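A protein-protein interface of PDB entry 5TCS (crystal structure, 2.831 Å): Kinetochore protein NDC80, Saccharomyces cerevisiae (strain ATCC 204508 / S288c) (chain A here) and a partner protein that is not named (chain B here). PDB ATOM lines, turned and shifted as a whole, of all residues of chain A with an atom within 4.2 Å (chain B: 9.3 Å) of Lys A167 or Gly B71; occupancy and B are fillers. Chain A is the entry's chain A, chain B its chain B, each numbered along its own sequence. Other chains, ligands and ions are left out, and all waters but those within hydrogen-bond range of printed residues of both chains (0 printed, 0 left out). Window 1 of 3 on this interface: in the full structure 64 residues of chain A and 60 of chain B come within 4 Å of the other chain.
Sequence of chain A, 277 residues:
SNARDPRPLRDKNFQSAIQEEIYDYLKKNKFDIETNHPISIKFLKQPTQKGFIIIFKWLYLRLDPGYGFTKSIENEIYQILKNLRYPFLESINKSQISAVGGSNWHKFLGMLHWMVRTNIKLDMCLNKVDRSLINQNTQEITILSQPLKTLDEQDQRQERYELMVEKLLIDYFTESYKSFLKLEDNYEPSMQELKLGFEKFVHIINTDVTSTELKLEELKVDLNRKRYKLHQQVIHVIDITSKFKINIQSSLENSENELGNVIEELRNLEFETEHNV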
ATOM      1  N   ASN A 137     -32.414  19.563  15.395  1.00  0.00           N
ATOM      2  CA  ASN A 137     -31.502  19.739  16.518  1.00  0.00           C
ATOM      3  C   ASN A 137     -32.046  19.165  17.816  1.00  0.00           C
ATOM      4  O   ASN A 137     -31.284  19.039  18.782  1.00  0.00           O
ATOM      5  CB  ASN A 137     -31.175  21.220  16.711  1.00  0.00           C
ATOM      6  CG  ASN A 137     -29.907  21.635  15.988  1.00  0.00           C
ATOM      7  OD1 ASN A 137     -29.694  21.283  14.825  1.00  0.00           O
ATOM      8  ND2 ASN A 137     -29.047  22.374  16.682  1.00  0.00           N
ATOM      9  N   GLU A 140     -33.544  13.782  18.046  1.00  0.00           N
ATOM     10  CA  GLU A 140     -32.904  12.682  18.758  1.00  0.00           C
ATOM     11  C   GLU A 140     -33.343  12.641  20.218  1.00  0.00           C
ATOM     12  O   GLU A 140     -33.974  11.674  20.660  1.00  0.00           O
ATOM     13  CB  GLU A 140     -31.381  12.796  18.653  1.00  0.00           C
ATOM     14  CG  GLU A 140     -30.818  12.358  17.306  1.00  0.00           C
ATOM     15  CD  GLU A 140     -30.559  13.522  16.367  1.00  0.00           C
ATOM     16  OE1 GLU A 140     -30.021  14.554  16.826  1.00  0.00           O
ATOM     17  OE2 GLU A 140     -30.892  13.405  15.168  1.00  0.00           O
ATOM     18  N   LEU A 163     -24.974  10.490  16.803  1.00  0.00           N
ATOM     19  CA  LEU A 163     -25.380  11.660  16.032  1.00  0.00           C
ATOM     20  C   LEU A 163     -25.557  12.875  16.937  1.00  0.00           C
ATOM     21  O   LEU A 163     -25.077  13.969  16.621  1.00  0.00           O
ATOM     22  CB  LEU A 163     -26.671  11.352  15.272  1.00  0.00           C
ATOM     23  CG  LEU A 163     -26.939  12.116  13.974  1.00  0.00           C
ATOM     24  CD1 LEU A 163     -28.179  11.555  13.306  1.00  0.00           C
ATOM     25  CD2 LEU A 163     -27.096  13.607  14.212  1.00  0.00           C
ATOM     26  N   MET A 164     -26.243  12.703  18.063  1.00  0.00           N
ATOM     27  CA  MET A 164     -26.464  13.787  19.017  1.00  0.00           C
ATOM     28  C   MET A 164     -25.146  14.475  19.390  1.00  0.00           C
ATOM     29  O   MET A 164     -24.952  15.690  19.157  1.00  0.00           O
ATOM     30  CB  MET A 164     -27.150  13.240  20.273  1.00  0.00           C
ATOM     31  CG  MET A 164     -27.707  14.298  21.209  1.00  0.00           C
ATOM     32  SD  MET A 164     -28.407  13.531  22.868  1.00  0.00           S
ATOM     33  CE  MET A 164     -29.880  12.504  22.117  1.00  0.00           C
ATOM     34  N   VAL A 165     -24.229  13.695  19.963  1.00  0.00           N
ATOM     35  CA  VAL A 165     -22.948  14.266  20.372  1.00  0.00           C
ATOM     36  C   VAL A 165     -22.204  14.818  19.166  1.00  0.00           C
ATOM     37  O   VAL A 165     -21.501  15.832  19.263  1.00  0.00           O
ATOM     38  CB  VAL A 165     -22.112  13.214  21.122  1.00  0.00           C
ATOM     39  CG1 VAL A 165     -20.617  13.541  21.070  1.00  0.00           C
ATOM     40  CG2 VAL A 165     -22.569  13.121  22.569  1.00  0.00           C
ATOM     41  N   GLU A 166     -22.331  14.162  18.010  1.00  0.00           N
ATOM     42  CA  GLU A 166     -21.686  14.702  16.820  1.00  0.00           C
ATOM     43  C   GLU A 166     -22.173  16.116  16.541  1.00  0.00           C
ATOM     44  O   GLU A 166     -21.376  16.998  16.208  1.00  0.00           O
ATOM     45  CB  GLU A 166     -21.937  13.809  15.608  1.00  0.00           C
ATOM     46  CG  GLU A 166     -21.184  14.280  14.360  1.00  0.00           C
ATOM     47  CD  GLU A 166     -21.420  13.394  13.159  1.00  0.00           C
ATOM     48  OE1 GLU A 166     -21.920  12.263  13.341  1.00  0.00           O
ATOM     49  OE2 GLU A 166     -21.106  13.835  12.031  1.00  0.00           O
ATOM     50  N   LYS A 167     -23.479  16.354  16.679  1.00  0.00           N
ATOM     51  CA  LYS A 167     -24.011  17.687  16.423  1.00  0.00           C
ATOM     52  C   LYS A 167     -23.497  18.687  17.449  1.00  0.00           C
ATOM     53  O   LYS A 167     -23.164  19.828  17.101  1.00  0.00           O
ATOM     54  CB  LYS A 167     -25.538  17.653  16.415  1.00  0.00           C
ATOM     55  CG  LYS A 167     -26.119  16.795  15.303  1.00  0.00           C
ATOM     56  CD  LYS A 167     -27.585  17.128  15.027  1.00  0.00           C
ATOM     57  CE  LYS A 167     -27.830  17.532  13.574  1.00  0.00           C
ATOM     58  NZ  LYS A 167     -28.637  18.781  13.473  1.00  0.00           N
ATOM     59  N   LEU A 168     -23.424  18.284  18.720  1.00  0.00           N
ATOM     60  CA  LEU A 168     -22.825  19.164  19.723  1.00  0.00           C
ATOM     61  C   LEU A 168     -21.405  19.561  19.322  1.00  0.00           C
ATOM     62  O   LEU A 168     -21.056  20.752  19.289  1.00  0.00           O
ATOM     63  CB  LEU A 168     -22.826  18.476  21.091  1.00  0.00           C
ATOM     64  CG  LEU A 168     -24.178  18.294  21.786  1.00  0.00           C
ATOM     65  CD1 LEU A 168     -23.990  17.589  23.124  1.00  0.00           C
ATOM     66  CD2 LEU A 168     -24.878  19.633  21.988  1.00  0.00           C
ATOM     67  N   LEU A 169     -20.573  18.566  19.003  1.00  0.00           N
ATOM     68  CA  LEU A 169     -19.201  18.844  18.599  1.00  0.00           C
ATOM     69  C   LEU A 169     -19.159  19.745  17.372  1.00  0.00           C
ATOM     70  O   LEU A 169     -18.298  20.624  17.273  1.00  0.00           O
ATOM     71  CB  LEU A 169     -18.467  17.531  18.329  1.00  0.00           C
ATOM     72  CG  LEU A 169     -18.195  16.669  19.563  1.00  0.00           C
ATOM     73  CD1 LEU A 169     -17.720  15.293  19.157  1.00  0.00           C
ATOM     74  CD2 LEU A 169     -17.163  17.323  20.453  1.00  0.00           C
ATOM     75  N   ILE A 170     -20.075  19.541  16.425  1.00  0.00           N
ATOM     76  CA  ILE A 170     -20.114  20.383  15.233  1.00  0.00           C
ATOM     77  C   ILE A 170     -20.379  21.832  15.616  1.00  0.00           C
ATOM     78  O   ILE A 170     -19.741  22.754  15.091  1.00  0.00           O
ATOM     79  CB  ILE A 170     -21.166  19.853  14.238  1.00  0.00           C
ATOM     80  CG1 ILE A 170     -20.654  18.571  13.574  1.00  0.00           C
ATOM     81  CG2 ILE A 170     -21.503  20.911  13.179  1.00  0.00           C
ATOM     82  CD1 ILE A 170     -21.643  17.919  12.627  1.00  0.00           C
ATOM     83  N   ASP A 171     -21.328  22.061  16.527  1.00  0.00           N
ATOM     84  CA  ASP A 171     -21.580  23.423  16.990  1.00  0.00           C
ATOM     85  C   ASP A 171     -20.315  24.033  17.582  1.00  0.00           C
ATOM     86  O   ASP A 171     -19.919  25.154  17.224  1.00  0.00           O
ATOM     87  CB  ASP A 171     -22.713  23.431  18.017  1.00  0.00           C
ATOM     88  CG  ASP A 171     -24.063  23.126  17.400  1.00  0.00           C
ATOM     89  OD1 ASP A 171     -24.203  23.278  16.168  1.00  0.00           O
ATOM     90  OD2 ASP A 171     -24.985  22.740  18.152  1.00  0.00           O
ATOM     91  N   LYS B  63     -22.269  19.138  -1.841  1.00  0.00           N
ATOM     92  CA  LYS B  63     -23.250  18.392  -1.062  1.00  0.00           C
ATOM     93  C   LYS B  63     -22.561  17.458  -0.076  1.00  0.00           C
ATOM     94  O   LYS B  63     -22.908  17.420   1.110  1.00  0.00           O
ATOM     95  CB  LYS B  63     -24.171  17.609  -2.000  1.00  0.00           C
ATOM     96  CG  LYS B  63     -25.436  18.353  -2.403  1.00  0.00           C
ATOM     97  CD  LYS B  63     -26.060  17.740  -3.648  1.00  0.00           C
ATOM     98  CE  LYS B  63     -27.547  18.044  -3.751  1.00  0.00           C
ATOM     99  NZ  LYS B  63     -28.151  17.501  -5.004  1.00  0.00           N
ATOM    100  N   GLN B  64     -21.574  16.696  -0.552  1.00  0.00           N
ATOM    101  CA  GLN B  64     -20.827  15.804   0.329  1.00  0.00           C
ATOM    102  C   GLN B  64     -20.167  16.579   1.461  1.00  0.00           C
ATOM    103  O   GLN B  64     -20.222  16.166   2.626  1.00  0.00           O
ATOM    104  CB  GLN B  64     -19.780  15.034  -0.480  1.00  0.00           C
ATOM    105  CG  GLN B  64     -20.110  13.566  -0.687  1.00  0.00           C
ATOM    106  CD  GLN B  64     -19.171  12.885  -1.665  1.00  0.00           C
ATOM    107  OE1 GLN B  64     -19.608  12.161  -2.561  1.00  0.00           O
ATOM    108  NE2 GLN B  64     -17.872  13.104  -1.492  1.00  0.00           N
ATOM    109  N   ILE B  65     -19.551  17.719   1.138  1.00  0.00           N
ATOM    110  CA  ILE B  65     -18.826  18.498   2.141  1.00  0.00           C
ATOM    111  C   ILE B  65     -19.782  18.998   3.218  1.00  0.00           C
ATOM    112  O   ILE B  65     -19.595  18.742   4.413  1.00  0.00           O
ATOM    113  CB  ILE B  65     -18.073  19.658   1.464  1.00  0.00           C
ATOM    114  CG1 ILE B  65     -16.881  19.105   0.679  1.00  0.00           C
ATOM    115  CG2 ILE B  65     -17.616  20.697   2.493  1.00  0.00           C
ATOM    116  CD1 ILE B  65     -16.175  20.128  -0.183  1.00  0.00           C
ATOM    117  N   ILE B  66     -20.813  19.736   2.807  1.00  0.00           N
ATOM    118  CA  ILE B  66     -21.773  20.274   3.766  1.00  0.00           C
ATOM    119  C   ILE B  66     -22.397  19.153   4.584  1.00  0.00           C
ATOM    120  O   ILE B  66     -22.544  19.266   5.806  1.00  0.00           O
ATOM    121  CB  ILE B  66     -22.838  21.106   3.028  1.00  0.00           C
ATOM    122  CG1 ILE B  66     -22.233  22.432   2.575  1.00  0.00           C
ATOM    123  CG2 ILE B  66     -24.048  21.365   3.917  1.00  0.00           C
ATOM    124  CD1 ILE B  66     -22.882  23.002   1.346  1.00  0.00           C
ATOM    125  N   GLU B  67     -22.775  18.055   3.930  1.00  0.00           N
ATOM    126  CA  GLU B  67     -23.398  16.955   4.656  1.00  0.00           C
ATOM    127  C   GLU B  67     -22.450  16.356   5.684  1.00  0.00           C
ATOM    128  O   GLU B  67     -22.893  15.919   6.752  1.00  0.00           O
ATOM    129  CB  GLU B  67     -23.879  15.882   3.679  1.00  0.00           C
ATOM    130  CG  GLU B  67     -25.256  16.173   3.108  1.00  0.00           C
ATOM    131  CD  GLU B  67     -25.661  15.222   1.997  1.00  0.00           C
ATOM    132  OE1 GLU B  67     -24.823  14.397   1.573  1.00  0.00           O
ATOM    133  OE2 GLU B  67     -26.828  15.297   1.554  1.00  0.00           O
ATOM    134  N   ASN B  68     -21.149  16.336   5.396  1.00  0.00           N
ATOM    135  CA  ASN B  68     -20.206  15.731   6.329  1.00  0.00           C
ATOM    136  C   ASN B  68     -19.852  16.676   7.474  1.00  0.00           C
ATOM    137  O   ASN B  68     -19.728  16.238   8.622  1.00  0.00           O
ATOM    138  CB  ASN B  68     -18.939  15.300   5.594  1.00  0.00           C
ATOM    139  CG  ASN B  68     -17.984  14.541   6.488  1.00  0.00           C
ATOM    140  OD1 ASN B  68     -18.092  13.324   6.640  1.00  0.00           O
ATOM    141  ND2 ASN B  68     -17.044  15.256   7.091  1.00  0.00           N
ATOM    142  N   PHE B  69     -19.683  17.968   7.189  1.00  0.00           N
ATOM    143  CA  PHE B  69     -19.276  18.917   8.219  1.00  0.00           C
ATOM    144  C   PHE B  69     -20.456  19.459   9.021  1.00  0.00           C
ATOM    145  O   PHE B  69     -20.349  19.604  10.242  1.00  0.00           O
ATOM    146  CB  PHE B  69     -18.504  20.086   7.591  1.00  0.00           C
ATOM    147  CG  PHE B  69     -17.092  19.747   7.178  1.00  0.00           C
ATOM    148  CD1 PHE B  69     -16.517  18.527   7.498  1.00  0.00           C
ATOM    149  CD2 PHE B  69     -16.334  20.665   6.474  1.00  0.00           C
ATOM    150  CE1 PHE B  69     -15.225  18.232   7.115  1.00  0.00           C
ATOM    151  CE2 PHE B  69     -15.038  20.372   6.093  1.00  0.00           C
ATOM    152  CZ  PHE B  69     -14.486  19.154   6.414  1.00  0.00           C
ATOM    153  N   MET B  70     -21.573  19.767   8.369  1.00  0.00           N
ATOM    154  CA  MET B  70     -22.737  20.289   9.081  1.00  0.00           C
ATOM    155  C   MET B  70     -23.555  19.167   9.714  1.00  0.00           C
ATOM    156  O   MET B  70     -24.439  19.422  10.529  1.00  0.00           O
ATOM    157  CB  MET B  70     -23.625  21.111   8.144  1.00  0.00           C
ATOM    158  CG  MET B  70     -23.100  22.515   7.866  1.00  0.00           C
ATOM    159  SD  MET B  70     -24.371  23.615   6.866  1.00  0.00           S
ATOM    160  CE  MET B  70     -24.424  25.179   8.034  1.00  0.00           C
ATOM    161  N   GLY B  71     -23.257  17.926   9.340  1.00  0.00           N
ATOM    162  CA  GLY B  71     -23.957  16.782   9.889  1.00  0.00           C
ATOM    163  C   GLY B  71     -25.453  16.848   9.662  1.00  0.00           C
ATOM    164  O   GLY B  71     -26.241  16.605  10.581  1.00  0.00           O
ATOM    165  N   ILE B  72     -25.855  17.179   8.435  1.00  0.00           N
ATOM    166  CA  ILE B  72     -27.258  17.279   8.057  1.00  0.00           C
ATOM    167  C   ILE B  72     -27.425  16.668   6.672  1.00  0.00           C
ATOM    168  O   ILE B  72     -26.452  16.319   6.003  1.00  0.00           O
ATOM    169  CB  ILE B  72     -27.764  18.736   8.070  1.00  0.00           C
ATOM    170  CG1 ILE B  72     -26.964  19.586   7.076  1.00  0.00           C
ATOM    171  CG2 ILE B  72     -27.672  19.320   9.472  1.00  0.00           C
ATOM    172  CD1 ILE B  72     -27.632  19.741   5.730  1.00  0.00           C
ATOM    173  N   SER B  73     -28.680  16.548   6.244  1.00  0.00           N
ATOM    174  CA  SER B  73     -29.029  15.961   4.955  1.00  0.00           C
ATOM    175  C   SER B  73     -29.649  17.030   4.067  1.00  0.00           C
ATOM    176  O   SER B  73     -30.643  17.660   4.449  1.00  0.00           O
ATOM    177  CB  SER B  73     -29.992  14.787   5.134  1.00  0.00           C
ATOM    178  OG  SER B  73     -30.676  14.505   3.928  1.00  0.00           O
ATOM    179  N   VAL B  74     -29.068  17.230   2.881  1.00  0.00           N
ATOM    180  CA  VAL B  74     -29.578  18.252   1.972  1.00  0.00           C
ATOM    181  C   VAL B  74     -30.937  17.841   1.418  1.00  0.00           C
ATOM    182  O   VAL B  74     -31.866  18.655   1.351  1.00  0.00           O
ATOM    183  CB  VAL B  74     -28.567  18.520   0.843  1.00  0.00           C
ATOM    184  CG1 VAL B  74     -29.011  19.703  -0.004  1.00  0.00           C
ATOM    185  CG2 VAL B  74     -27.186  18.771   1.412  1.00  0.00           C
ATOM    186  N   SER B  76     -33.182  16.193   2.796  1.00  0.00           N
ATOM    187  CA  SER B  76     -34.186  16.430   3.827  1.00  0.00           C
ATOM    188  C   SER B  76     -34.606  17.895   3.858  1.00  0.00           C
ATOM    189  O   SER B  76     -35.801  18.213   3.828  1.00  0.00           O
ATOM    190  CB  SER B  76     -33.641  15.997   5.188  1.00  0.00           C
ATOM    191  OG  SER B  76     -34.547  16.325   6.225  1.00  0.00           O
ATOM    192  N   LEU B  77     -33.632  18.805   3.926  1.00  0.00           N
ATOM    193  CA  LEU B  77     -33.955  20.227   3.982  1.00  0.00           C
ATOM    194  C   LEU B  77     -34.727  20.665   2.744  1.00  0.00           C
ATOM    195  O   LEU B  77     -35.655  21.477   2.840  1.00  0.00           O
ATOM    196  CB  LEU B  77     -32.676  21.048   4.132  1.00  0.00           C
ATOM    197  CG  LEU B  77     -31.860  20.802   5.402  1.00  0.00           C
ATOM    198  CD1 LEU B  77     -30.615  21.663   5.380  1.00  0.00           C
ATOM    199  CD2 LEU B  77     -32.677  21.085   6.656  1.00  0.00           C
ATOM    200  N   PHE B 114     -22.935  28.121   4.897  1.00  0.00           N
ATOM    201  CA  PHE B 114     -21.791  27.311   5.296  1.00  0.00           C
ATOM    202  C   PHE B 114     -20.480  28.042   5.028  1.00  0.00           C
ATOM    203  O   PHE B 114     -19.634  28.171   5.919  1.00  0.00           O
ATOM    204  CB  PHE B 114     -21.827  25.974   4.566  1.00  0.00           C
ATOM    205  CG  PHE B 114     -20.555  25.185   4.671  1.00  0.00           C
ATOM    206  CD1 PHE B 114     -20.255  24.472   5.819  1.00  0.00           C
ATOM    207  CD2 PHE B 114     -19.667  25.137   3.611  1.00  0.00           C
ATOM    208  CE1 PHE B 114     -19.091  23.740   5.909  1.00  0.00           C
ATOM    209  CE2 PHE B 114     -18.501  24.404   3.698  1.00  0.00           C
ATOM    210  CZ  PHE B 114     -18.212  23.706   4.848  1.00  0.00           C
ATOM    211  N   TYR B 146     -10.616  24.843   7.508  1.00  0.00           N
ATOM    212  CA  TYR B 146     -11.568  24.501   8.557  1.00  0.00           C
ATOM    213  C   TYR B 146     -11.372  23.066   9.029  1.00  0.00           C
ATOM    214  O   TYR B 146     -11.421  22.787  10.233  1.00  0.00           O
ATOM    215  CB  TYR B 146     -12.996  24.711   8.064  1.00  0.00           C
ATOM    216  CG  TYR B 146     -14.035  24.294   9.074  1.00  0.00           C
ATOM    217  CD1 TYR B 146     -14.080  24.878  10.330  1.00  0.00           C
ATOM    218  CD2 TYR B 146     -14.971  23.317   8.773  1.00  0.00           C
ATOM    219  CE1 TYR B 146     -15.027  24.501  11.260  1.00  0.00           C
ATOM    220  CE2 TYR B 146     -15.922  22.933   9.695  1.00  0.00           C
ATOM    221  CZ  TYR B 146     -15.946  23.529  10.937  1.00  0.00           C
ATOM    222  OH  TYR B 146     -16.895  23.150  11.858  1.00  0.00           O
ATOM    223  N   ARG B 150     -10.629  22.004  12.901  1.00  0.00           N
ATOM    224  CA  ARG B 150     -11.453  21.011  13.581  1.00  0.00           C
ATOM    225  C   ARG B 150     -10.600  19.875  14.128  1.00  0.00           C
ATOM    226  O   ARG B 150     -10.733  19.488  15.295  1.00  0.00           O
ATOM    227  CB  ARG B 150     -12.504  20.473  12.614  1.00  0.00           C
ATOM    228  CG  ARG B 150     -13.383  19.374  13.184  1.00  0.00           C
ATOM    229  CD  ARG B 150     -14.025  18.562  12.075  1.00  0.00           C
ATOM    230  NE  ARG B 150     -13.022  17.933  11.221  1.00  0.00           N
ATOM    231  CZ  ARG B 150     -13.299  17.174  10.167  1.00  0.00           C
ATOM    232  NH1 ARG B 150     -14.560  16.932   9.823  1.00  0.00           N
ATOM    233  NH2 ARG B 150     -12.307  16.652   9.457  1.00  0.00           N
ATOM    234  N   MET B 154     -10.588  18.549  18.063  1.00  0.00           N
ATOM    235  CA  MET B 154     -10.952  17.218  18.537  1.00  0.00           C
ATOM    236  C   MET B 154     -10.233  16.871  19.833  1.00  0.00           C
ATOM    237  O   MET B 154     -10.844  16.363  20.774  1.00  0.00           O
ATOM    238  CB  MET B 154     -10.638  16.164  17.476  1.00  0.00           C
ATOM    239  CG  MET B 154     -11.795  15.865  16.548  1.00  0.00           C
ATOM    240  SD  MET B 154     -13.330  15.146  17.511  1.00  0.00           S
ATOM    241  CE  MET B 154     -14.588  15.015  16.024  1.00  0.00           C
ATOM    242  N   ILE B 161     -15.820  12.222  23.946  1.00  0.00           N
ATOM    243  CA  ILE B 161     -15.893  11.008  23.135  1.00  0.00           C
ATOM    244  C   ILE B 161     -15.679   9.775  24.002  1.00  0.00           C
ATOM    245  O   ILE B 161     -16.445   8.805  23.939  1.00  0.00           O
ATOM    246  CB  ILE B 161     -14.865  11.075  21.990  1.00  0.00           C
ATOM    247  CG1 ILE B 161     -15.199  12.221  21.028  1.00  0.00           C
ATOM    248  CG2 ILE B 161     -14.790   9.745  21.244  1.00  0.00           C
ATOM    249  CD1 ILE B 161     -16.529  12.073  20.308  1.00  0.00           C
ATOM    250  N   MET B 164     -18.660   9.033  26.308  1.00  0.00           N
ATOM    251  CA  MET B 164     -19.711   8.478  25.468  1.00  0.00           C
ATOM    252  C   MET B 164     -19.473   6.997  25.217  1.00  0.00           C
ATOM    253  O   MET B 164     -20.284   6.148  25.599  1.00  0.00           O
ATOM    254  CB  MET B 164     -19.769   9.223  24.136  1.00  0.00           C
ATOM    255  CG  MET B 164     -20.483   8.466  23.030  1.00  0.00           C
ATOM    256  SD  MET B 164     -20.338   9.334  21.309  1.00  0.00           S
ATOM    257  CE  MET B 164     -22.165   9.932  21.250  1.00  0.00           C
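OD1 of Asn A137 is in hydrogen-bond range of NZ of Lys A167 (3.0 Å).
Among the printed residues, merely in contact across the chains: Ile A170 with Phe B69 (3.2 Å), Val A165 with Met B164 (3.3 Å), Lys A167 with Gly B71 (3.5 Å), Leu A169 with Ile B161 (3.6 Å), Ile A170 with Gly B71 (3.7 Å) and Ile A170 with Met B70 (3.7 Å).
Of chain B, only Gly B71 (3.5 Å) comes within 4 Å of Lys A167. Gly B71 touches just these residues of chain A: Lys A167 (3.5 Å) and Ile A170 (3.7 Å). Ile A170 touches three residues of chain B. Printed residues of chain A within 4 Å of Met B164: Val A165 (3.3 Å). Printed residues of chain A within 4 Å of Met B70: Ile A170. Of the printed residues of chain B, Val A165 touches Met B164 (3.3 Å). Of the printed residues of chain A, Ile B161 touches Leu A169. Printed residues of chain B within 4 Å of Leu A169: Ile B161. The nearest residue of chain B that does not touch Lys A167 is Ile B72 (4.2 Å).
Printed residues of chain A that touch a printed residue of chain B: Val A165, Lys A167, Leu A169 and Ile A170. Along chain A the printed residues that touch a printed residue of chain B span positions 165 to 170. Of the 20 printed residues of chain B, 5 touch a printed residue of chain A. Printed residues of chain B that touch a printed residue of chain A: Phe B69, Met B70, Gly B71, Ile B161 and Met B164. Hydrophobic or aromatic side chains of chain B that line the printed part of chain A: Ile B161 and Met B164.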
